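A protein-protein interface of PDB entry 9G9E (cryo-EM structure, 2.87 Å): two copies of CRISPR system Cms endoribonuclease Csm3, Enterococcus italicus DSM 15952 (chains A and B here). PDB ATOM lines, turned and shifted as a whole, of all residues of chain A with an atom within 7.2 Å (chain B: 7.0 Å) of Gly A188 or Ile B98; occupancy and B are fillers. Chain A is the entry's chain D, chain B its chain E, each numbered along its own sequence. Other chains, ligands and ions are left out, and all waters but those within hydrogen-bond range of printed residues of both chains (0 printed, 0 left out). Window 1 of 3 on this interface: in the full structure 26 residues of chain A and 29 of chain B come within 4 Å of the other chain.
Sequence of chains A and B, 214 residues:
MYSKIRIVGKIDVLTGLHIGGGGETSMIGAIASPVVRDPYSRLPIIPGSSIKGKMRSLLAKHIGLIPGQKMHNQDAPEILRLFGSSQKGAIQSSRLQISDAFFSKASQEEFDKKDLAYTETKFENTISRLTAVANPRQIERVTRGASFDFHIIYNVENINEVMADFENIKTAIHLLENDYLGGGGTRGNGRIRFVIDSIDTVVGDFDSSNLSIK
The side-chain hydroxyl (OG) of Ser B94 sits at hydrogen-bond distance from the backbone carbonyl oxygen (O) of Leu B96 (2.8 Å). The backbone carbonyl oxygen of Phe B83 lies within hydrogen-bond range of the side-chain hydroxyl of Ser B94, at 3.2 Å. The side-chain hydroxyl (OG1) of Thr A15 lies within hydrogen-bond range of the backbone NH (N) of Arg A191 (3.1 Å). The side-chain amide oxygen (OD1) of Asn A189 is in hydrogen-bond range of the guanidinium group (NH2) of Arg A141 (2.9 Å). The backbone NH (N) of Gly B48 sits at hydrogen-bond distance from the side-chain carboxylate (OD1) of Asp B100, at 2.8 Å. The guanidinium group (NH2) of Arg A141 sits at hydrogen-bond distance from the backbone carbonyl oxygen (O) of Gly A188 (3.3 Å).
Among the printed residues, pairs that only touch across the chains: Thr A15 with Ser B99 (3.4 Å), Thr A15 with Phe B102 (3.7 Å), Lys A122 with Pro B47 (3.7 Å), Tyr A180 with Gln B97 (3.3 Å), Thr A186 with Ser B94 (3.6 Å), Thr A186 with Leu B96 (3.7 Å), Thr A186 with Gln B97 (3.8 Å), Arg A187 with Gly B48 (3.8 Å), Arg A187 with Lys B52 (3.8 Å), Arg A187 with Ile B98 (3.5 Å), Gly A188 with Ser B99 (3.7 Å) and Arg A191 with His B151 (3.8 Å).
Of the 14 printed residues of chain A, 8 touch a printed residue of chain B. Hydrophobic or aromatic side chains of chain A within 4 Å of the printed part of chain B: Tyr A180. Among the printed residues, Asp or Glu carboxylates within 4 Å of a Lys or Arg side-chain nitrogen of the other chain: Arg A141 with Asp B100 (2.9 Å).
No position is printed for both chains.
Of the printed residues of chain B, Arg A141 touches Asp B100 (2.9 Å). Gly A188 touches three residues of chain B. Gly A190 touches none of the printed residues of chain B. Ile B51 touches none of the printed residues of chain A. Of the printed residues of chain A, Lys B52 touches Thr A186 (3.0 Å) and Arg A187 (3.8 Å). Printed residues of chain A within 4 Å of Ser B94: Thr A186 (3.6 Å). Of the printed residues of chain A, His B151 touches Arg A191. The nearest residue of chain A that does not touch Ile B98 is Gly A185 (4.7 Å). The nearest printed residue of chain A that does not touch Asp B100 is Arg A187 (4.1 Å).
The side-chain hydroxyl of Thr A186 is in hydrogen-bond range of the side-chain amino group of Lys B52, at 3.0 Å. The backbone carbonyl oxygen of Thr A186 lies within hydrogen-bond range of the backbone NH of Ile B98 (3.2 Å). The backbone carbonyl oxygen of Arg A187 lies within hydrogen-bond range of the backbone NH of Ser B49, at 3.3 Å. The side-chain carboxylate (OD1) of Asp B100 lies close to the backbone carbonyl oxygen (O) of Gly A188 (3.0 Å). NH1 of Arg A191 is in hydrogen-bond range of OG of Ser B99 (2.9 Å). The side-chain carboxylate (OD2) of Asp B100 is in salt-bridge range of the guanidinium group (NH2) of Arg A141 (2.9 Å). O of Ile B98 sits at hydrogen-bond distance from N of Gly A188. The side-chain amino group (NZ) of Lys A122 lies within hydrogen-bond range of the side-chain hydroxyl (OG) of Ser B49, 3.2 Å away.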
ATOM      1  N   THR A  15     -31.646  26.683 -15.581  1.00  0.00           N
ATOM      2  CA  THR A  15     -30.361  27.364 -15.618  1.00  0.00           C
ATOM      3  C   THR A  15     -30.563  28.755 -16.201  1.00  0.00           C
ATOM      4  O   THR A  15     -31.474  28.975 -17.004  1.00  0.00           O
ATOM      5  CB  THR A  15     -29.316  26.601 -16.454  1.00  0.00           C
ATOM      6  OG1 THR A  15     -29.614  26.746 -17.849  1.00  0.00           O
ATOM      7  CG2 THR A  15     -29.296  25.123 -16.093  1.00  0.00           C
ATOM      8  N   GLY A  16     -29.696  29.685 -15.796  1.00  0.00           N
ATOM      9  CA  GLY A  16     -29.806  31.089 -16.157  1.00  0.00           C
ATOM     10  C   GLY A  16     -30.212  31.365 -17.590  1.00  0.00           C
ATOM     11  O   GLY A  16     -29.544  30.927 -18.530  1.00  0.00           O
ATOM     12  N   LEU A  17     -31.306  32.102 -17.765  1.00  0.00           N
ATOM     13  CA  LEU A  17     -31.920  32.320 -19.067  1.00  0.00           C
ATOM     14  C   LEU A  17     -31.587  33.716 -19.573  1.00  0.00           C
ATOM     15  O   LEU A  17     -31.861  34.710 -18.892  1.00  0.00           O
ATOM     16  CB  LEU A  17     -33.437  32.139 -18.983  1.00  0.00           C
ATOM     17  CG  LEU A  17     -34.255  32.627 -20.178  1.00  0.00           C
ATOM     18  CD1 LEU A  17     -34.215  31.614 -21.308  1.00  0.00           C
ATOM     19  CD2 LEU A  17     -35.684  32.914 -19.757  1.00  0.00           C
ATOM     20  N   LYS A 122     -23.188  37.148 -15.558  1.00  0.00           N
ATOM     21  CA  LYS A 122     -22.291  36.022 -15.773  1.00  0.00           C
ATOM     22  C   LYS A 122     -21.048  36.494 -16.513  1.00  0.00           C
ATOM     23  O   LYS A 122     -21.146  37.176 -17.540  1.00  0.00           O
ATOM     24  CB  LYS A 122     -22.983  34.909 -16.559  1.00  0.00           C
ATOM     25  CG  LYS A 122     -22.212  33.599 -16.569  1.00  0.00           C
ATOM     26  CD  LYS A 122     -22.667  32.694 -17.698  1.00  0.00           C
ATOM     27  CE  LYS A 122     -22.028  31.320 -17.590  1.00  0.00           C
ATOM     28  NZ  LYS A 122     -20.557  31.407 -17.379  1.00  0.00           N
ATOM     29  N   ARG A 141     -28.338  37.212 -17.159  1.00  0.00           N
ATOM     30  CA  ARG A 141     -29.252  36.081 -17.174  1.00  0.00           C
ATOM     31  C   ARG A 141     -30.331  36.281 -16.122  1.00  0.00           C
ATOM     32  O   ARG A 141     -30.215  37.126 -15.235  1.00  0.00           O
ATOM     33  CB  ARG A 141     -28.527  34.752 -16.914  1.00  0.00           C
ATOM     34  CG  ARG A 141     -27.318  34.498 -17.789  1.00  0.00           C
ATOM     35  CD  ARG A 141     -26.298  33.655 -17.048  1.00  0.00           C
ATOM     36  NE  ARG A 141     -26.620  32.234 -17.101  1.00  0.00           N
ATOM     37  CZ  ARG A 141     -26.130  31.325 -16.270  1.00  0.00           C
ATOM     38  NH1 ARG A 141     -25.285  31.653 -15.306  1.00  0.00           N
ATOM     39  NH2 ARG A 141     -26.497  30.055 -16.409  1.00  0.00           N
ATOM     40  N   TYR A 180     -32.808  24.428 -24.707  1.00  0.00           N
ATOM     41  CA  TYR A 180     -32.772  25.738 -24.075  1.00  0.00           C
ATOM     42  C   TYR A 180     -33.829  26.637 -24.710  1.00  0.00           C
ATOM     43  O   TYR A 180     -34.525  26.250 -25.651  1.00  0.00           O
ATOM     44  CB  TYR A 180     -31.379  26.369 -24.182  1.00  0.00           C
ATOM     45  CG  TYR A 180     -30.710  26.293 -25.545  1.00  0.00           C
ATOM     46  CD1 TYR A 180     -30.286  25.081 -26.080  1.00  0.00           C
ATOM     47  CD2 TYR A 180     -30.502  27.442 -26.293  1.00  0.00           C
ATOM     48  CE1 TYR A 180     -29.677  25.020 -27.318  1.00  0.00           C
ATOM     49  CE2 TYR A 180     -29.894  27.390 -27.530  1.00  0.00           C
ATOM     50  CZ  TYR A 180     -29.484  26.178 -28.038  1.00  0.00           C
ATOM     51  OH  TYR A 180     -28.879  26.125 -29.271  1.00  0.00           O
ATOM     52  N   GLY A 184     -26.995  31.452 -25.463  1.00  0.00           N
ATOM     53  CA  GLY A 184     -26.175  30.303 -25.779  1.00  0.00           C
ATOM     54  C   GLY A 184     -26.415  29.164 -24.815  1.00  0.00           C
ATOM     55  O   GLY A 184     -25.803  29.101 -23.746  1.00  0.00           O
ATOM     56  N   GLY A 185     -27.300  28.244 -25.197  1.00  0.00           N
ATOM     57  CA  GLY A 185     -27.659  27.129 -24.347  1.00  0.00           C
ATOM     58  C   GLY A 185     -26.781  25.917 -24.477  1.00  0.00           C
ATOM     59  O   GLY A 185     -26.837  25.026 -23.624  1.00  0.00           O
ATOM     60  N   THR A 186     -25.967  25.854 -25.528  1.00  0.00           N
ATOM     61  CA  THR A 186     -24.941  24.826 -25.612  1.00  0.00           C
ATOM     62  C   THR A 186     -23.847  25.029 -24.575  1.00  0.00           C
ATOM     63  O   THR A 186     -23.062  24.105 -24.335  1.00  0.00           O
ATOM     64  CB  THR A 186     -24.335  24.804 -27.015  1.00  0.00           C
ATOM     65  OG1 THR A 186     -23.800  26.097 -27.325  1.00  0.00           O
ATOM     66  CG2 THR A 186     -25.398  24.449 -28.040  1.00  0.00           C
ATOM     67  N   ARG A 187     -23.785  26.208 -23.959  1.00  0.00           N
ATOM     68  CA  ARG A 187     -22.862  26.509 -22.873  1.00  0.00           C
ATOM     69  C   ARG A 187     -23.611  26.687 -21.554  1.00  0.00           C
ATOM     70  O   ARG A 187     -23.265  27.536 -20.731  1.00  0.00           O
ATOM     71  CB  ARG A 187     -22.034  27.748 -23.200  1.00  0.00           C
ATOM     72  CG  ARG A 187     -21.219  27.617 -24.477  1.00  0.00           C
ATOM     73  CD  ARG A 187     -20.495  28.911 -24.823  1.00  0.00           C
ATOM     74  NE  ARG A 187     -21.414  30.008 -25.105  1.00  0.00           N
ATOM     75  CZ  ARG A 187     -22.122  30.132 -26.221  1.00  0.00           C
ATOM     76  NH1 ARG A 187     -22.046  29.239 -27.192  1.00  0.00           N
ATOM     77  NH2 ARG A 187     -22.927  31.181 -26.364  1.00  0.00           N
ATOM     78  N   GLY A 188     -24.652  25.883 -21.346  1.00  0.00           N
ATOM     79  CA  GLY A 188     -25.372  25.852 -20.088  1.00  0.00           C
ATOM     80  C   GLY A 188     -26.209  27.068 -19.751  1.00  0.00           C
ATOM     81  O   GLY A 188     -26.138  27.580 -18.629  1.00  0.00           O
ATOM     82  N   ASN A 189     -27.010  27.541 -20.702  1.00  0.00           N
ATOM     83  CA  ASN A 189     -27.937  28.638 -20.472  1.00  0.00           C
ATOM     84  C   ASN A 189     -29.326  28.261 -20.968  1.00  0.00           C
ATOM     85  O   ASN A 189     -29.482  27.409 -21.846  1.00  0.00           O
ATOM     86  CB  ASN A 189     -27.480  29.922 -21.178  1.00  0.00           C
ATOM     87  CG  ASN A 189     -26.382  30.644 -20.426  1.00  0.00           C
ATOM     88  OD1 ASN A 189     -26.081  30.320 -19.280  1.00  0.00           O
ATOM     89  ND2 ASN A 189     -25.778  31.635 -21.071  1.00  0.00           N
ATOM     90  N   GLY A 190     -30.339  28.893 -20.382  1.00  0.00           N
ATOM     91  CA  GLY A 190     -31.681  28.846 -20.923  1.00  0.00           C
ATOM     92  C   GLY A 190     -32.459  27.571 -20.689  1.00  0.00           C
ATOM     93  O   GLY A 190     -33.541  27.421 -21.268  1.00  0.00           O
ATOM     94  N   ARG A 191     -31.957  26.647 -19.874  1.00  0.00           N
ATOM     95  CA  ARG A 191     -32.731  25.452 -19.563  1.00  0.00           C
ATOM     96  C   ARG A 191     -33.977  25.833 -18.778  1.00  0.00           C
ATOM     97  O   ARG A 191     -33.922  26.668 -17.871  1.00  0.00           O
ATOM     98  CB  ARG A 191     -31.892  24.451 -18.772  1.00  0.00           C
ATOM     99  CG  ARG A 191     -30.936  23.636 -19.619  1.00  0.00           C
ATOM    100  CD  ARG A 191     -30.208  22.612 -18.772  1.00  0.00           C
ATOM    101  NE  ARG A 191     -31.135  21.705 -18.107  1.00  0.00           N
ATOM    102  CZ  ARG A 191     -30.895  21.098 -16.953  1.00  0.00           C
ATOM    103  NH1 ARG A 191     -29.765  21.287 -16.294  1.00  0.00           N
ATOM    104  NH2 ARG A 191     -31.814  20.280 -16.447  1.00  0.00           N
ATOM    105  N   PRO B  47     -19.914  26.314 -14.248  1.00  0.00           N
ATOM    106  CA  PRO B  47     -20.620  26.730 -15.464  1.00  0.00           C
ATOM    107  C   PRO B  47     -20.404  25.736 -16.596  1.00  0.00           C
ATOM    108  O   PRO B  47     -19.309  25.199 -16.775  1.00  0.00           O
ATOM    109  CB  PRO B  47     -20.000  28.096 -15.786  1.00  0.00           C
ATOM    110  CG  PRO B  47     -19.379  28.553 -14.507  1.00  0.00           C
ATOM    111  CD  PRO B  47     -18.925  27.311 -13.811  1.00  0.00           C
ATOM    112  N   GLY B  48     -21.467  25.493 -17.364  1.00  0.00           N
ATOM    113  CA  GLY B  48     -21.357  24.622 -18.518  1.00  0.00           C
ATOM    114  C   GLY B  48     -20.461  25.173 -19.603  1.00  0.00           C
ATOM    115  O   GLY B  48     -19.902  24.398 -20.387  1.00  0.00           O
ATOM    116  N   SER B  49     -20.308  26.498 -19.659  1.00  0.00           N
ATOM    117  CA  SER B  49     -19.364  27.096 -20.593  1.00  0.00           C
ATOM    118  C   SER B  49     -17.940  26.658 -20.286  1.00  0.00           C
ATOM    119  O   SER B  49     -17.165  26.372 -21.203  1.00  0.00           O
ATOM    120  CB  SER B  49     -19.481  28.619 -20.555  1.00  0.00           C
ATOM    121  OG  SER B  49     -19.461  29.098 -19.224  1.00  0.00           O
ATOM    122  N   SER B  50     -17.579  26.587 -19.001  1.00  0.00           N
ATOM    123  CA  SER B  50     -16.240  26.140 -18.628  1.00  0.00           C
ATOM    124  C   SER B  50     -15.992  24.706 -19.080  1.00  0.00           C
ATOM    125  O   SER B  50     -14.950  24.401 -19.674  1.00  0.00           O
ATOM    126  CB  SER B  50     -16.047  26.260 -17.115  1.00  0.00           C
ATOM    127  OG  SER B  50     -16.079  27.610 -16.694  1.00  0.00           O
ATOM    128  N   ILE B  51     -16.946  23.813 -18.809  1.00  0.00           N
ATOM    129  CA  ILE B  51     -16.786  22.410 -19.183  1.00  0.00           C
ATOM    130  C   ILE B  51     -16.691  22.273 -20.696  1.00  0.00           C
ATOM    131  O   ILE B  51     -15.816  21.573 -21.220  1.00  0.00           O
ATOM    132  CB  ILE B  51     -17.942  21.566 -18.618  1.00  0.00           C
ATOM    133  CG1 ILE B  51     -18.256  21.977 -17.178  1.00  0.00           C
ATOM    134  CG2 ILE B  51     -17.608  20.084 -18.696  1.00  0.00           C
ATOM    135  CD1 ILE B  51     -19.598  21.485 -16.685  1.00  0.00           C
ATOM    136  N   LYS B  52     -17.593  22.943 -21.418  1.00  0.00           N
ATOM    137  CA  LYS B  52     -17.594  22.835 -22.873  1.00  0.00           C
ATOM    138  C   LYS B  52     -16.308  23.392 -23.467  1.00  0.00           C
ATOM    139  O   LYS B  52     -15.725  22.786 -24.372  1.00  0.00           O
ATOM    140  CB  LYS B  52     -18.812  23.550 -23.456  1.00  0.00           C
ATOM    141  CG  LYS B  52     -19.086  23.196 -24.906  1.00  0.00           C
ATOM    142  CD  LYS B  52     -20.038  24.177 -25.560  1.00  0.00           C
ATOM    143  CE  LYS B  52     -20.432  23.702 -26.948  1.00  0.00           C
ATOM    144  NZ  LYS B  52     -21.090  24.774 -27.741  1.00  0.00           N
ATOM    145  N   GLY B  53     -15.840  24.536 -22.963  1.00  0.00           N
ATOM    146  CA  GLY B  53     -14.618  25.119 -23.486  1.00  0.00           C
ATOM    147  C   GLY B  53     -13.394  24.271 -23.204  1.00  0.00           C
ATOM    148  O   GLY B  53     -12.544  24.090 -24.080  1.00  0.00           O
ATOM    149  N   MET B  55     -13.330  20.984 -22.648  1.00  0.00           N
ATOM    150  CA  MET B  55     -13.425  19.784 -23.471  1.00  0.00           C
ATOM    151  C   MET B  55     -13.072  20.080 -24.921  1.00  0.00           C
ATOM    152  O   MET B  55     -12.335  19.316 -25.555  1.00  0.00           O
ATOM    153  CB  MET B  55     -14.830  19.191 -23.371  1.00  0.00           C
ATOM    154  CG  MET B  55     -15.085  18.406 -22.096  1.00  0.00           C
ATOM    155  SD  MET B  55     -16.817  17.944 -21.898  1.00  0.00           S
ATOM    156  CE  MET B  55     -17.106  17.045 -23.418  1.00  0.00           C
ATOM    157  N   PHE B  83     -19.062  20.483 -31.029  1.00  0.00           N
ATOM    158  CA  PHE B  83     -19.238  21.684 -30.223  1.00  0.00           C
ATOM    159  C   PHE B  83     -19.784  22.870 -31.007  1.00  0.00           C
ATOM    160  O   PHE B  83     -20.049  23.916 -30.405  1.00  0.00           O
ATOM    161  CB  PHE B  83     -17.909  22.071 -29.567  1.00  0.00           C
ATOM    162  CG  PHE B  83     -17.279  20.958 -28.779  1.00  0.00           C
ATOM    163  CD1 PHE B  83     -17.636  20.740 -27.459  1.00  0.00           C
ATOM    164  CD2 PHE B  83     -16.334  20.129 -29.359  1.00  0.00           C
ATOM    165  CE1 PHE B  83     -17.062  19.718 -26.732  1.00  0.00           C
ATOM    166  CE2 PHE B  83     -15.757  19.104 -28.636  1.00  0.00           C
ATOM    167  CZ  PHE B  83     -16.121  18.898 -27.321  1.00  0.00           C
ATOM    168  N   SER B  94     -24.357  23.044 -32.669  1.00  0.00           N
ATOM    169  CA  SER B  94     -23.618  22.210 -31.731  1.00  0.00           C
ATOM    170  C   SER B  94     -24.474  21.042 -31.264  1.00  0.00           C
ATOM    171  O   SER B  94     -25.604  21.230 -30.801  1.00  0.00           O
ATOM    172  CB  SER B  94     -23.161  23.042 -30.536  1.00  0.00           C
ATOM    173  OG  SER B  94     -22.632  22.215 -29.517  1.00  0.00           O
ATOM    174  N   ARG B  95     -23.933  19.829 -31.388  1.00  0.00           N
ATOM    175  CA  ARG B  95     -24.635  18.647 -30.907  1.00  0.00           C
ATOM    176  C   ARG B  95     -24.554  18.512 -29.392  1.00  0.00           C
ATOM    177  O   ARG B  95     -25.506  18.037 -28.765  1.00  0.00           O
ATOM    178  CB  ARG B  95     -24.076  17.391 -31.576  1.00  0.00           C
ATOM    179  CG  ARG B  95     -24.206  17.397 -33.088  1.00  0.00           C
ATOM    180  CD  ARG B  95     -23.883  16.039 -33.682  1.00  0.00           C
ATOM    181  NE  ARG B  95     -23.767  16.100 -35.135  1.00  0.00           N
ATOM    182  CZ  ARG B  95     -23.585  15.046 -35.917  1.00  0.00           C
ATOM    183  NH1 ARG B  95     -23.504  13.823 -35.422  1.00  0.00           N
ATOM    184  NH2 ARG B  95     -23.481  15.223 -37.231  1.00  0.00           N
ATOM    185  N   LEU B  96     -23.441  18.922 -28.792  1.00  0.00           N
ATOM    186  CA  LEU B  96     -23.257  18.822 -27.351  1.00  0.00           C
ATOM    187  C   LEU B  96     -23.764  20.083 -26.667  1.00  0.00           C
ATOM    188  O   LEU B  96     -23.363  21.195 -27.024  1.00  0.00           O
ATOM    189  CB  LEU B  96     -21.784  18.598 -27.008  1.00  0.00           C
ATOM    190  CG  LEU B  96     -21.262  17.165 -27.097  1.00  0.00           C
ATOM    191  CD1 LEU B  96     -19.776  17.125 -26.786  1.00  0.00           C
ATOM    192  CD2 LEU B  96     -22.035  16.255 -26.159  1.00  0.00           C
ATOM    193  N   GLN B  97     -24.638  19.904 -25.681  1.00  0.00           N
ATOM    194  CA  GLN B  97     -25.118  20.986 -24.829  1.00  0.00           C
ATOM    195  C   GLN B  97     -24.753  20.619 -23.398  1.00  0.00           C
ATOM    196  O   GLN B  97     -25.367  19.722 -22.810  1.00  0.00           O
ATOM    197  CB  GLN B  97     -26.623  21.187 -24.983  1.00  0.00           C
ATOM    198  CG  GLN B  97     -27.079  21.407 -26.414  1.00  0.00           C
ATOM    199  CD  GLN B  97     -28.584  21.524 -26.534  1.00  0.00           C
ATOM    200  OE1 GLN B  97     -29.112  21.800 -27.610  1.00  0.00           O
ATOM    201  NE2 GLN B  97     -29.284  21.311 -25.427  1.00  0.00           N
ATOM    202  N   ILE B  98     -23.745  21.294 -22.855  1.00  0.00           N
ATOM    203  CA  ILE B  98     -23.252  21.034 -21.509  1.00  0.00           C
ATOM    204  C   ILE B  98     -23.895  22.045 -20.572  1.00  0.00           C
ATOM    205  O   ILE B  98     -23.675  23.253 -20.706  1.00  0.00           O
ATOM    206  CB  ILE B  98     -21.720  21.121 -21.444  1.00  0.00           C
ATOM    207  CG1 ILE B  98     -21.095  20.603 -22.742  1.00  0.00           C
ATOM    208  CG2 ILE B  98     -21.193  20.349 -20.244  1.00  0.00           C
ATOM    209  CD1 ILE B  98     -21.012  19.099 -22.829  1.00  0.00           C
ATOM    210  N   SER B  99     -24.676  21.554 -19.618  1.00  0.00           N
ATOM    211  CA  SER B  99     -25.396  22.415 -18.696  1.00  0.00           C
ATOM    212  C   SER B  99     -24.535  22.738 -17.478  1.00  0.00           C
ATOM    213  O   SER B  99     -23.517  22.096 -17.212  1.00  0.00           O
ATOM    214  CB  SER B  99     -26.706  21.755 -18.267  1.00  0.00           C
ATOM    215  OG  SER B  99     -27.383  22.536 -17.298  1.00  0.00           O
ATOM    216  N   ASP B 100     -24.955  23.762 -16.738  1.00  0.00           N
ATOM    217  CA  ASP B 100     -24.284  24.114 -15.494  1.00  0.00           C
ATOM    218  C   ASP B 100     -24.371  22.959 -14.506  1.00  0.00           C
ATOM    219  O   ASP B 100     -25.443  22.384 -14.294  1.00  0.00           O
ATOM    220  CB  ASP B 100     -24.912  25.370 -14.888  1.00  0.00           C
ATOM    221  CG  ASP B 100     -24.696  26.606 -15.740  1.00  0.00           C
ATOM    222  OD1 ASP B 100     -24.066  26.499 -16.811  1.00  0.00           O
ATOM    223  OD2 ASP B 100     -25.159  27.691 -15.334  1.00  0.00           O
ATOM    224  N   ALA B 101     -23.238  22.619 -13.901  1.00  0.00           N
ATOM    225  CA  ALA B 101     -23.183  21.574 -12.888  1.00  0.00           C
ATOM    226  C   ALA B 101     -23.414  22.204 -11.521  1.00  0.00           C
ATOM    227  O   ALA B 101     -22.584  22.987 -11.044  1.00  0.00           O
ATOM    228  CB  ALA B 101     -21.844  20.841 -12.933  1.00  0.00           C
ATOM    229  N   PHE B 102     -24.535  21.863 -10.896  1.00  0.00           N
ATOM    230  CA  PHE B 102     -24.919  22.447  -9.621  1.00  0.00           C
ATOM    231  C   PHE B 102     -24.438  21.579  -8.468  1.00  0.00           C
ATOM    232  O   PHE B 102     -24.313  20.358  -8.595  1.00  0.00           O
ATOM    233  CB  PHE B 102     -26.437  22.618  -9.545  1.00  0.00           C
ATOM    234  CG  PHE B 102     -27.005  23.477 -10.637  1.00  0.00           C
ATOM    235  CD1 PHE B 102     -26.832  24.851 -10.617  1.00  0.00           C
ATOM    236  CD2 PHE B 102     -27.710  22.911 -11.686  1.00  0.00           C
ATOM    237  CE1 PHE B 102     -27.354  25.642 -11.622  1.00  0.00           C
ATOM    238  CE2 PHE B 102     -28.233  23.697 -12.692  1.00  0.00           C
ATOM    239  CZ  PHE B 102     -28.055  25.065 -12.660  1.00  0.00           C
ATOM    240  N   PHE B 150     -23.790  16.910 -13.135  1.00  0.00           N
ATOM    241  CA  PHE B 150     -23.563  17.332 -14.510  1.00  0.00           C
ATOM    242  C   PHE B 150     -24.593  16.694 -15.431  1.00  0.00           C
ATOM    243  O   PHE B 150     -24.944  15.518 -15.281  1.00  0.00           O
ATOM    244  CB  PHE B 150     -22.128  17.016 -14.962  1.00  0.00           C
ATOM    245  CG  PHE B 150     -21.948  15.674 -15.629  1.00  0.00           C
ATOM    246  CD1 PHE B 150     -22.226  15.498 -16.978  1.00  0.00           C
ATOM    247  CD2 PHE B 150     -21.451  14.599 -14.914  1.00  0.00           C
ATOM    248  CE1 PHE B 150     -22.046  14.270 -17.584  1.00  0.00           C
ATOM    249  CE2 PHE B 150     -21.265  13.371 -15.517  1.00  0.00           C
ATOM    250  CZ  PHE B 150     -21.564  13.206 -16.852  1.00  0.00           C
ATOM    251  N   HIS B 151     -25.082  17.494 -16.378  1.00  0.00           N
ATOM    252  CA  HIS B 151     -26.130  17.104 -17.309  1.00  0.00           C
ATOM    253  C   HIS B 151     -25.738  17.557 -18.707  1.00  0.00           C
ATOM    254  O   HIS B 151     -25.474  18.745 -18.925  1.00  0.00           O
ATOM    255  CB  HIS B 151     -27.473  17.717 -16.894  1.00  0.00           C
ATOM    256  CG  HIS B 151     -28.549  17.589 -17.925  1.00  0.00           C
ATOM    257  ND1 HIS B 151     -28.810  18.574 -18.853  1.00  0.00           N
ATOM    258  CD2 HIS B 151     -29.440  16.599 -18.168  1.00  0.00           C
ATOM    259  CE1 HIS B 151     -29.810  18.194 -19.626  1.00  0.00           C
ATOM    260  NE2 HIS B 151     -30.210  16.999 -19.232  1.00  0.00           N
ATOM    261  N   ILE B 152     -25.695  16.616 -19.647  1.00  0.00           N
ATOM    262  CA  ILE B 152     -25.293  16.882 -21.022  1.00  0.00           C
ATOM    263  C   ILE B 152     -26.372  16.351 -21.954  1.00  0.00           C
ATOM    264  O   ILE B 152     -26.918  15.265 -21.730  1.00  0.00           O
ATOM    265  CB  ILE B 152     -23.927  16.239 -21.347  1.00  0.00           C
ATOM    266  CG1 ILE B 152     -22.838  16.800 -20.431  1.00  0.00           C
ATOM    267  CG2 ILE B 152     -23.559  16.453 -22.805  1.00  0.00           C
ATOM    268  CD1 ILE B 152     -21.495  16.123 -20.595  1.00  0.00           C
ATOM    269  N   ILE B 153     -26.696  17.122 -22.987  1.00  0.00           N
ATOM    270  CA  ILE B 153     -27.659  16.706 -24.002  1.00  0.00           C
ATOM    271  C   ILE B 153     -26.933  16.612 -25.336  1.00  0.00           C
ATOM    272  O   ILE B 153     -26.349  17.597 -25.804  1.00  0.00           O
ATOM    273  CB  ILE B 153     -28.852  17.671 -24.092  1.00  0.00           C
ATOM    274  CG1 ILE B 153     -29.818  17.429 -22.932  1.00  0.00           C
ATOM    275  CG2 ILE B 153     -29.573  17.507 -25.422  1.00  0.00           C
ATOM    276  CD1 ILE B 153     -30.687  16.202 -23.101  1.00  0.00           C
ATOM    277  N   ILE B 169     -16.255  12.318 -27.711  1.00  0.00           N
ATOM    278  CA  ILE B 169     -16.635  12.762 -26.374  1.00  0.00           C
ATOM    279  C   ILE B 169     -15.857  11.980 -25.331  1.00  0.00           C
ATOM    280  O   ILE B 169     -15.279  12.559 -24.402  1.00  0.00           O
ATOM    281  CB  ILE B 169     -18.154  12.624 -26.168  1.00  0.00           C
ATOM    282  CG1 ILE B 169     -18.916  13.360 -27.269  1.00  0.00           C
ATOM    283  CG2 ILE B 169     -18.554  13.169 -24.807  1.00  0.00           C
ATOM    284  CD1 ILE B 169     -20.404  13.090 -27.262  1.00  0.00           C
ATOM    285  N   PHE B 194     -15.109  12.210 -13.643  1.00  0.00           N
ATOM    286  CA  PHE B 194     -16.465  12.065 -14.156  1.00  0.00           C
ATOM    287  C   PHE B 194     -16.962  10.650 -13.901  1.00  0.00           C
ATOM    288  O   PHE B 194     -16.305   9.679 -14.291  1.00  0.00           O
ATOM    289  CB  PHE B 194     -16.519  12.374 -15.653  1.00  0.00           C
ATOM    290  CG  PHE B 194     -16.478  13.840 -15.972  1.00  0.00           C
ATOM    291  CD1 PHE B 194     -15.309  14.563 -15.825  1.00  0.00           C
ATOM    292  CD2 PHE B 194     -17.613  14.491 -16.423  1.00  0.00           C
ATOM    293  CE1 PHE B 194     -15.271  15.910 -16.118  1.00  0.00           C
ATOM    294  CE2 PHE B 194     -17.583  15.839 -16.718  1.00  0.00           C
ATOM    295  CZ  PHE B 194     -16.411  16.549 -16.566  1.00  0.00           C
